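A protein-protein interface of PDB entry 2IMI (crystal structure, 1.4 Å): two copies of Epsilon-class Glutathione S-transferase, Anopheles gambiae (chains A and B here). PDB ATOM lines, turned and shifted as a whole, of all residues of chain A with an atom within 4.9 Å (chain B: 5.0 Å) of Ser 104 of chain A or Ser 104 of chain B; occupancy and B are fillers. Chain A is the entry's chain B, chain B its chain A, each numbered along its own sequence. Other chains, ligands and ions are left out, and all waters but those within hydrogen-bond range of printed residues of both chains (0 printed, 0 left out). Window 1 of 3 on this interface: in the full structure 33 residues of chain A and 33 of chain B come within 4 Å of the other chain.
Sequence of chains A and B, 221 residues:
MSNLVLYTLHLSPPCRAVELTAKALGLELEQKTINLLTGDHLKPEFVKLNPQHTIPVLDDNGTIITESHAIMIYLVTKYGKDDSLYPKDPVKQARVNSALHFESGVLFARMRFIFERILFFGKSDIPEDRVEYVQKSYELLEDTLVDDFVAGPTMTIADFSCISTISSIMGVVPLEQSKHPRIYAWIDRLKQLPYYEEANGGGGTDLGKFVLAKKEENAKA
His 69 of chain A touches His 101 of chain B, and with the chains exchanged His 101 of chain A touches His 69 of chain B. His 101 of chain A touches its own counterpart, His 101 of chain B. Ser 104 of chain B touches its own counterpart, Ser 104 of chain A. Gly 105 of chain A touches Ala 109 of chain B, and with the chains exchanged Ala 109 of chain A touches Gly 105 of chain B. 10 positions are printed for both chains.
Among the printed residues, merely in contact across the chains: His 69 of chain A with His 101 of chain B (3.5 Å), Leu 100 of chain A with His 101 of chain B (3.5 Å), His 101 of chain A with His 69 of chain B (3.5 Å), His 101 of chain A with Leu 100 of chain B (3.5 Å), Ser 104 of chain A with Gly 105 of chain B (3.4 Å), Gly 105 of chain A with Ser 104 of chain B (3.4 Å), Gly 105 of chain A with Ala 109 of chain B (3.8 Å), Ala 109 of chain A with Gly 105 of chain B (3.9 Å) and Ala 109 of chain A with Ala 109 of chain B (3.6 Å).
Of the 11 printed residues of chain B, 6 touch a printed residue of chain A. Hydrophobic or aromatic side chains of chain A that line the printed part of chain B: His 69, Leu 100, His 101 and Ala 109. Among the printed residues, 13 pairs touch across the chains.
OG of Ser 104 of chain B lies within hydrogen-bond range of ND1 of His 101 of chain A (2.9 Å). ND1 of His 101 of chain B sits at hydrogen-bond distance from OG of Ser 104 of chain A. A ring nitrogen (NE2) of His 101 of chain B lies within hydrogen-bond range of a ring nitrogen (NE2) of His 101 of chain A (3.3 Å). OG of Ser 104 of chain B sits at hydrogen-bond distance from OG of Ser 104 of chain A (2.7 Å).
The side-chain carboxylate (OE1) of Glu 103 of chain B lies close to a ring nitrogen (NE2) of His 69 of chain B (3.1 Å). The backbone carbonyl oxygen (O) of Leu 100 of chain A is in hydrogen-bond range of the side-chain hydroxyl (OG) of Ser 104 of chain A (3.5 Å). The backbone carbonyl oxygen (O) of Ser 104 of chain A sits at hydrogen-bond distance from the backbone NH (N) of Ala 109 of chain A, at 3.4 Å. The backbone carbonyl oxygen (O) of His 101 of chain B lies within hydrogen-bond range of the side-chain hydroxyl (OG) of Ser 104 of chain B, 3.5 Å away. O of Ser 104 of chain B sits at hydrogen-bond distance from N of Ala 109 of chain B (3.3 Å). OE2 of Glu 103 of chain A is in hydrogen-bond range of NE2 of His 69 of chain A.
Printed residues of chain B within 4 Å of His 101 of chain A: His 69, Leu 100, His 101 and Ser 104. Ser 104 of chain A touches just these residues of chain B: His 101, Ser 104 and Gly 105. Of the printed residues of chain A, Leu 100 of chain B touches His 101 (3.5 Å). Printed residues of chain A within 4 Å of His 101 of chain B: His 69, Leu 100, His 101 and Ser 104. Phe 102 of chain B touches none of the printed residues of chain A. Ser 104 of chain B touches just these residues of chain A: His 101 (2.9 Å), Ser 104 (2.7 Å) and Gly 105 (3.4 Å). Printed residues of chain A within 4 Å of Gly 105 of chain B: Ser 104 and Ala 109. Leu 107 of chain B touches none of the printed residues of chain A. Of the printed residues of chain A, Ala 109 of chain B touches Gly 105 and Ala 109. The nearest printed residue of chain B that does not touch Ser 104 of chain A is Ala 109 of chain B (5.3 Å). The nearest printed residue of chain A that does not touch His 101 of chain B is Gly 105 of chain A (6.0 Å).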
ATOM      1  N   HIS A  69      10.012  12.934  22.241  1.00  0.00           N
ATOM      2  CA  HIS A  69      10.232  12.983  20.789  1.00  0.00           C
ATOM      3  C   HIS A  69      11.533  13.718  20.469  1.00  0.00           C
ATOM      4  O   HIS A  69      12.316  13.262  19.616  1.00  0.00           O
ATOM      5  CB  HIS A  69       9.028  13.599  20.060  1.00  0.00           C
ATOM      6  CG  HIS A  69       7.724  12.997  20.477  1.00  0.00           C
ATOM      7  ND1 HIS A  69       7.045  13.415  21.599  1.00  0.00           N
ATOM      8  CD2 HIS A  69       7.000  11.977  19.956  1.00  0.00           C
ATOM      9  CE1 HIS A  69       5.948  12.693  21.743  1.00  0.00           C
ATOM     10  NE2 HIS A  69       5.893  11.818  20.755  1.00  0.00           N
ATOM     11  N   LEU A 100       4.810  11.817  14.442  1.00  0.00           N
ATOM     12  CA  LEU A 100       5.216  12.159  15.816  1.00  0.00           C
ATOM     13  C   LEU A 100       4.250  13.119  16.486  1.00  0.00           C
ATOM     14  O   LEU A 100       3.949  12.963  17.673  1.00  0.00           O
ATOM     15  CB  LEU A 100       6.629  12.754  15.850  1.00  0.00           C
ATOM     16  CG  LEU A 100       7.759  11.791  15.478  1.00  0.00           C
ATOM     17  CD1 LEU A 100       9.055  12.555  15.291  1.00  0.00           C
ATOM     18  CD2 LEU A 100       7.935  10.710  16.531  1.00  0.00           C
ATOM     19  N   HIS A 101       3.783  14.116  15.741  1.00  0.00           N
ATOM     20  CA  HIS A 101       2.815  15.058  16.301  1.00  0.00           C
ATOM     21  C   HIS A 101       1.410  14.479  16.424  1.00  0.00           C
ATOM     22  O   HIS A 101       0.641  14.894  17.301  1.00  0.00           O
ATOM     23  CB  HIS A 101       2.856  16.382  15.543  1.00  0.00           C
ATOM     24  CG  HIS A 101       4.078  17.178  15.857  1.00  0.00           C
ATOM     25  ND1 HIS A 101       4.184  17.934  17.003  1.00  0.00           N
ATOM     26  CD2 HIS A 101       5.270  17.276  15.225  1.00  0.00           C
ATOM     27  CE1 HIS A 101       5.378  18.496  17.044  1.00  0.00           C
ATOM     28  NE2 HIS A 101       6.060  18.107  15.980  1.00  0.00           N
ATOM     29  N   PHE A 102       1.073  13.524  15.564  1.00  0.00           N
ATOM     30  CA  PHE A 102      -0.147  12.765  15.762  1.00  0.00           C
ATOM     31  C   PHE A 102      -0.043  12.037  17.107  1.00  0.00           C
ATOM     32  O   PHE A 102      -0.994  12.020  17.894  1.00  0.00           O
ATOM     33  CB  PHE A 102      -0.359  11.791  14.605  1.00  0.00           C
ATOM     34  CG  PHE A 102      -1.476  10.825  14.842  1.00  0.00           C
ATOM     35  CD1 PHE A 102      -2.794  11.249  14.767  1.00  0.00           C
ATOM     36  CD2 PHE A 102      -1.208   9.506  15.187  1.00  0.00           C
ATOM     37  CE1 PHE A 102      -3.847  10.363  15.003  1.00  0.00           C
ATOM     38  CE2 PHE A 102      -2.245   8.600  15.415  1.00  0.00           C
ATOM     39  CZ  PHE A 102      -3.567   9.042  15.335  1.00  0.00           C
ATOM     40  N   GLU A 103       1.110  11.446  17.395  1.00  0.00           N
ATOM     41  CA  GLU A 103       1.267  10.752  18.657  1.00  0.00           C
ATOM     42  C   GLU A 103       1.148  11.705  19.832  1.00  0.00           C
ATOM     43  O   GLU A 103       0.386  11.442  20.764  1.00  0.00           O
ATOM     44  CB  GLU A 103       2.580   9.976  18.720  1.00  0.00           C
ATOM     45  CG  GLU A 103       2.610   8.928  19.839  1.00  0.00           C
ATOM     46  CD  GLU A 103       2.885   9.497  21.224  1.00  0.00           C
ATOM     47  OE1 GLU A 103       2.400   8.913  22.215  1.00  0.00           O
ATOM     48  OE2 GLU A 103       3.593  10.518  21.346  1.00  0.00           O
ATOM     49  N   SER A 104       1.875  12.815  19.815  1.00  0.00           N
ATOM     50  CA  SER A 104       1.796  13.703  20.968  1.00  0.00           C
ATOM     51  C   SER A 104       0.437  14.391  21.083  1.00  0.00           C
ATOM     52  O   SER A 104      -0.146  14.452  22.173  1.00  0.00           O
ATOM     53  CB  SER A 104       2.953  14.707  21.011  1.00  0.00           C
ATOM     54  OG  SER A 104       2.990  15.512  19.853  1.00  0.00           O
ATOM     55  N   GLY A 105      -0.082  14.878  19.959  1.00  0.00           N
ATOM     56  CA  GLY A 105      -1.304  15.683  19.980  1.00  0.00           C
ATOM     57  C   GLY A 105      -2.600  14.899  20.053  1.00  0.00           C
ATOM     58  O   GLY A 105      -3.625  15.458  20.432  1.00  0.00           O
ATOM     59  N   VAL A 106      -2.567  13.624  19.672  1.00  0.00           N
ATOM     60  CA  VAL A 106      -3.787  12.813  19.619  1.00  0.00           C
ATOM     61  C   VAL A 106      -3.680  11.579  20.506  1.00  0.00           C
ATOM     62  O   VAL A 106      -4.408  11.475  21.487  1.00  0.00           O
ATOM     63  CB  VAL A 106      -4.176  12.424  18.161  1.00  0.00           C
ATOM     64  CG1 VAL A 106      -5.454  11.597  18.142  1.00  0.00           C
ATOM     65  CG2 VAL A 106      -4.373  13.672  17.304  1.00  0.00           C
ATOM     66  N   PHE A 108      -1.233  10.282  22.673  1.00  0.00           N
ATOM     67  CA  PHE A 108      -0.798  10.508  24.041  1.00  0.00           C
ATOM     68  C   PHE A 108      -1.741  11.446  24.778  1.00  0.00           C
ATOM     69  O   PHE A 108      -2.134  11.160  25.910  1.00  0.00           O
ATOM     70  CB  PHE A 108       0.630  11.064  24.095  1.00  0.00           C
ATOM     71  CG  PHE A 108       1.121  11.301  25.499  1.00  0.00           C
ATOM     72  CD1 PHE A 108       1.051  12.563  26.069  1.00  0.00           C
ATOM     73  CD2 PHE A 108       1.599  10.248  26.266  1.00  0.00           C
ATOM     74  CE1 PHE A 108       1.479  12.778  27.386  1.00  0.00           C
ATOM     75  CE2 PHE A 108       2.028  10.457  27.577  1.00  0.00           C
ATOM     76  CZ  PHE A 108       1.967  11.729  28.127  1.00  0.00           C
ATOM     77  N   ALA A 109      -2.109  12.560  24.151  1.00  0.00           N
ATOM     78  CA  ALA A 109      -2.941  13.533  24.842  1.00  0.00           C
ATOM     79  C   ALA A 109      -4.254  12.923  25.301  1.00  0.00           C
ATOM     80  O   ALA A 109      -4.723  13.190  26.419  1.00  0.00           O
ATOM     81  CB  ALA A 109      -3.206  14.728  23.954  1.00  0.00           C
ATOM     82  N   HIS B  69       3.249  21.269  12.103  1.00  0.00           N
ATOM     83  CA  HIS B  69       4.655  21.283  12.532  1.00  0.00           C
ATOM     84  C   HIS B  69       5.550  20.670  11.459  1.00  0.00           C
ATOM     85  O   HIS B  69       6.619  21.214  11.153  1.00  0.00           O
ATOM     86  CB  HIS B  69       4.837  20.594  13.888  1.00  0.00           C
ATOM     87  CG  HIS B  69       3.804  20.985  14.893  1.00  0.00           C
ATOM     88  ND1 HIS B  69       3.952  22.036  15.775  1.00  0.00           N
ATOM     89  CD2 HIS B  69       2.564  20.489  15.101  1.00  0.00           C
ATOM     90  CE1 HIS B  69       2.856  22.140  16.508  1.00  0.00           C
ATOM     91  NE2 HIS B  69       1.997  21.220  16.113  1.00  0.00           N
ATOM     92  N   LEU B 100       7.836  22.316  20.110  1.00  0.00           N
ATOM     93  CA  LEU B 100       6.814  21.946  19.132  1.00  0.00           C
ATOM     94  C   LEU B 100       5.886  20.866  19.684  1.00  0.00           C
ATOM     95  O   LEU B 100       4.668  20.935  19.487  1.00  0.00           O
ATOM     96  CB  LEU B 100       7.457  21.480  17.813  1.00  0.00           C
ATOM     97  CG  LEU B 100       8.190  22.551  16.991  1.00  0.00           C
ATOM     98  CD1 LEU B 100       9.007  21.878  15.903  1.00  0.00           C
ATOM     99  CD2 LEU B 100       7.229  23.564  16.388  1.00  0.00           C
ATOM    100  N   HIS B 101       6.447  19.900  20.408  1.00  0.00           N
ATOM    101  CA  HIS B 101       5.624  18.840  20.999  1.00  0.00           C
ATOM    102  C   HIS B 101       4.870  19.299  22.233  1.00  0.00           C
ATOM    103  O   HIS B 101       3.784  18.806  22.510  1.00  0.00           O
ATOM    104  CB  HIS B 101       6.446  17.582  21.249  1.00  0.00           C
ATOM    105  CG  HIS B 101       6.725  16.836  19.990  1.00  0.00           C
ATOM    106  ND1 HIS B 101       5.785  16.020  19.395  1.00  0.00           N
ATOM    107  CD2 HIS B 101       7.794  16.857  19.159  1.00  0.00           C
ATOM    108  CE1 HIS B 101       6.283  15.545  18.267  1.00  0.00           C
ATOM    109  NE2 HIS B 101       7.494  16.041  18.095  1.00  0.00           N
ATOM    110  N   PHE B 102       5.420  20.280  22.940  1.00  0.00           N
ATOM    111  CA  PHE B 102       4.656  20.927  24.000  1.00  0.00           C
ATOM    112  C   PHE B 102       3.410  21.576  23.393  1.00  0.00           C
ATOM    113  O   PHE B 102       2.299  21.477  23.942  1.00  0.00           O
ATOM    114  CB  PHE B 102       5.521  21.945  24.751  1.00  0.00           C
ATOM    115  CG  PHE B 102       4.751  22.774  25.739  1.00  0.00           C
ATOM    116  CD1 PHE B 102       4.334  22.216  26.935  1.00  0.00           C
ATOM    117  CD2 PHE B 102       4.439  24.094  25.468  1.00  0.00           C
ATOM    118  CE1 PHE B 102       3.614  22.965  27.851  1.00  0.00           C
ATOM    119  CE2 PHE B 102       3.716  24.851  26.388  1.00  0.00           C
ATOM    120  CZ  PHE B 102       3.311  24.280  27.571  1.00  0.00           C
ATOM    121  N   GLU B 103       3.573  22.210  22.239  1.00  0.00           N
ATOM    122  CA  GLU B 103       2.427  22.845  21.580  1.00  0.00           C
ATOM    123  C   GLU B 103       1.381  21.822  21.147  1.00  0.00           C
ATOM    124  O   GLU B 103       0.193  21.992  21.411  1.00  0.00           O
ATOM    125  CB  GLU B 103       2.837  23.744  20.401  1.00  0.00           C
ATOM    126  CG  GLU B 103       1.694  24.685  19.967  1.00  0.00           C
ATOM    127  CD  GLU B 103       0.653  24.056  19.032  1.00  0.00           C
ATOM    128  OE1 GLU B 103       0.943  23.029  18.388  1.00  0.00           O
ATOM    129  OE2 GLU B 103      -0.469  24.596  18.910  1.00  0.00           O
ATOM    130  N   SER B 104       1.798  20.760  20.472  1.00  0.00           N
ATOM    131  CA  SER B 104       0.803  19.792  20.013  1.00  0.00           C
ATOM    132  C   SER B 104       0.193  19.014  21.170  1.00  0.00           C
ATOM    133  O   SER B 104      -1.032  18.845  21.233  1.00  0.00           O
ATOM    134  CB  SER B 104       1.346  18.837  18.929  1.00  0.00           C
ATOM    135  OG  SER B 104       2.518  18.173  19.349  1.00  0.00           O
ATOM    136  N   GLY B 105       1.043  18.555  22.083  1.00  0.00           N
ATOM    137  CA  GLY B 105       0.605  17.649  23.136  1.00  0.00           C
ATOM    138  C   GLY B 105      -0.094  18.318  24.292  1.00  0.00           C
ATOM    139  O   GLY B 105      -0.912  17.682  24.954  1.00  0.00           O
ATOM    140  N   VAL B 106       0.224  19.592  24.538  1.00  0.00           N
ATOM    141  CA  VAL B 106      -0.308  20.315  25.698  1.00  0.00           C
ATOM    142  C   VAL B 106      -1.215  21.459  25.240  1.00  0.00           C
ATOM    143  O   VAL B 106      -2.426  21.407  25.465  1.00  0.00           O
ATOM    144  CB  VAL B 106       0.805  20.801  26.685  1.00  0.00           C
ATOM    145  CG1 VAL B 106       0.186  21.573  27.850  1.00  0.00           C
ATOM    146  CG2 VAL B 106       1.581  19.608  27.226  1.00  0.00           C
ATOM    147  N   LEU B 107      -0.649  22.484  24.606  1.00  0.00           N
ATOM    148  CA  LEU B 107      -1.438  23.682  24.306  1.00  0.00           C
ATOM    149  C   LEU B 107      -2.595  23.407  23.362  1.00  0.00           C
ATOM    150  O   LEU B 107      -3.755  23.691  23.673  1.00  0.00           O
ATOM    151  CB  LEU B 107      -0.550  24.780  23.720  1.00  0.00           C
ATOM    152  CG  LEU B 107       0.524  25.337  24.647  1.00  0.00           C
ATOM    153  CD1 LEU B 107       1.347  26.380  23.935  1.00  0.00           C
ATOM    154  CD2 LEU B 107      -0.105  25.942  25.894  1.00  0.00           C
ATOM    155  N   PHE B 108      -2.283  22.859  22.193  1.00  0.00           N
ATOM    156  CA  PHE B 108      -3.317  22.620  21.201  1.00  0.00           C
ATOM    157  C   PHE B 108      -4.272  21.527  21.652  1.00  0.00           C
ATOM    158  O   PHE B 108      -5.476  21.683  21.525  1.00  0.00           O
ATOM    159  CB  PHE B 108      -2.735  22.243  19.841  1.00  0.00           C
ATOM    160  CG  PHE B 108      -3.790  22.061  18.783  1.00  0.00           C
ATOM    161  CD1 PHE B 108      -4.216  20.789  18.437  1.00  0.00           C
ATOM    162  CD2 PHE B 108      -4.404  23.161  18.183  1.00  0.00           C
ATOM    163  CE1 PHE B 108      -5.225  20.604  17.485  1.00  0.00           C
ATOM    164  CE2 PHE B 108      -5.421  22.979  17.232  1.00  0.00           C
ATOM    165  CZ  PHE B 108      -5.814  21.700  16.882  1.00  0.00           C
ATOM    166  N   ALA B 109      -3.759  20.413  22.160  1.00  0.00           N
ATOM    167  CA  ALA B 109      -4.660  19.336  22.552  1.00  0.00           C
ATOM    168  C   ALA B 109      -5.688  19.823  23.570  1.00  0.00           C
ATOM    169  O   ALA B 109      -6.860  19.462  23.494  1.00  0.00           O
ATOM    170  CB  ALA B 109      -3.886  18.157  23.097  1.00  0.00           C
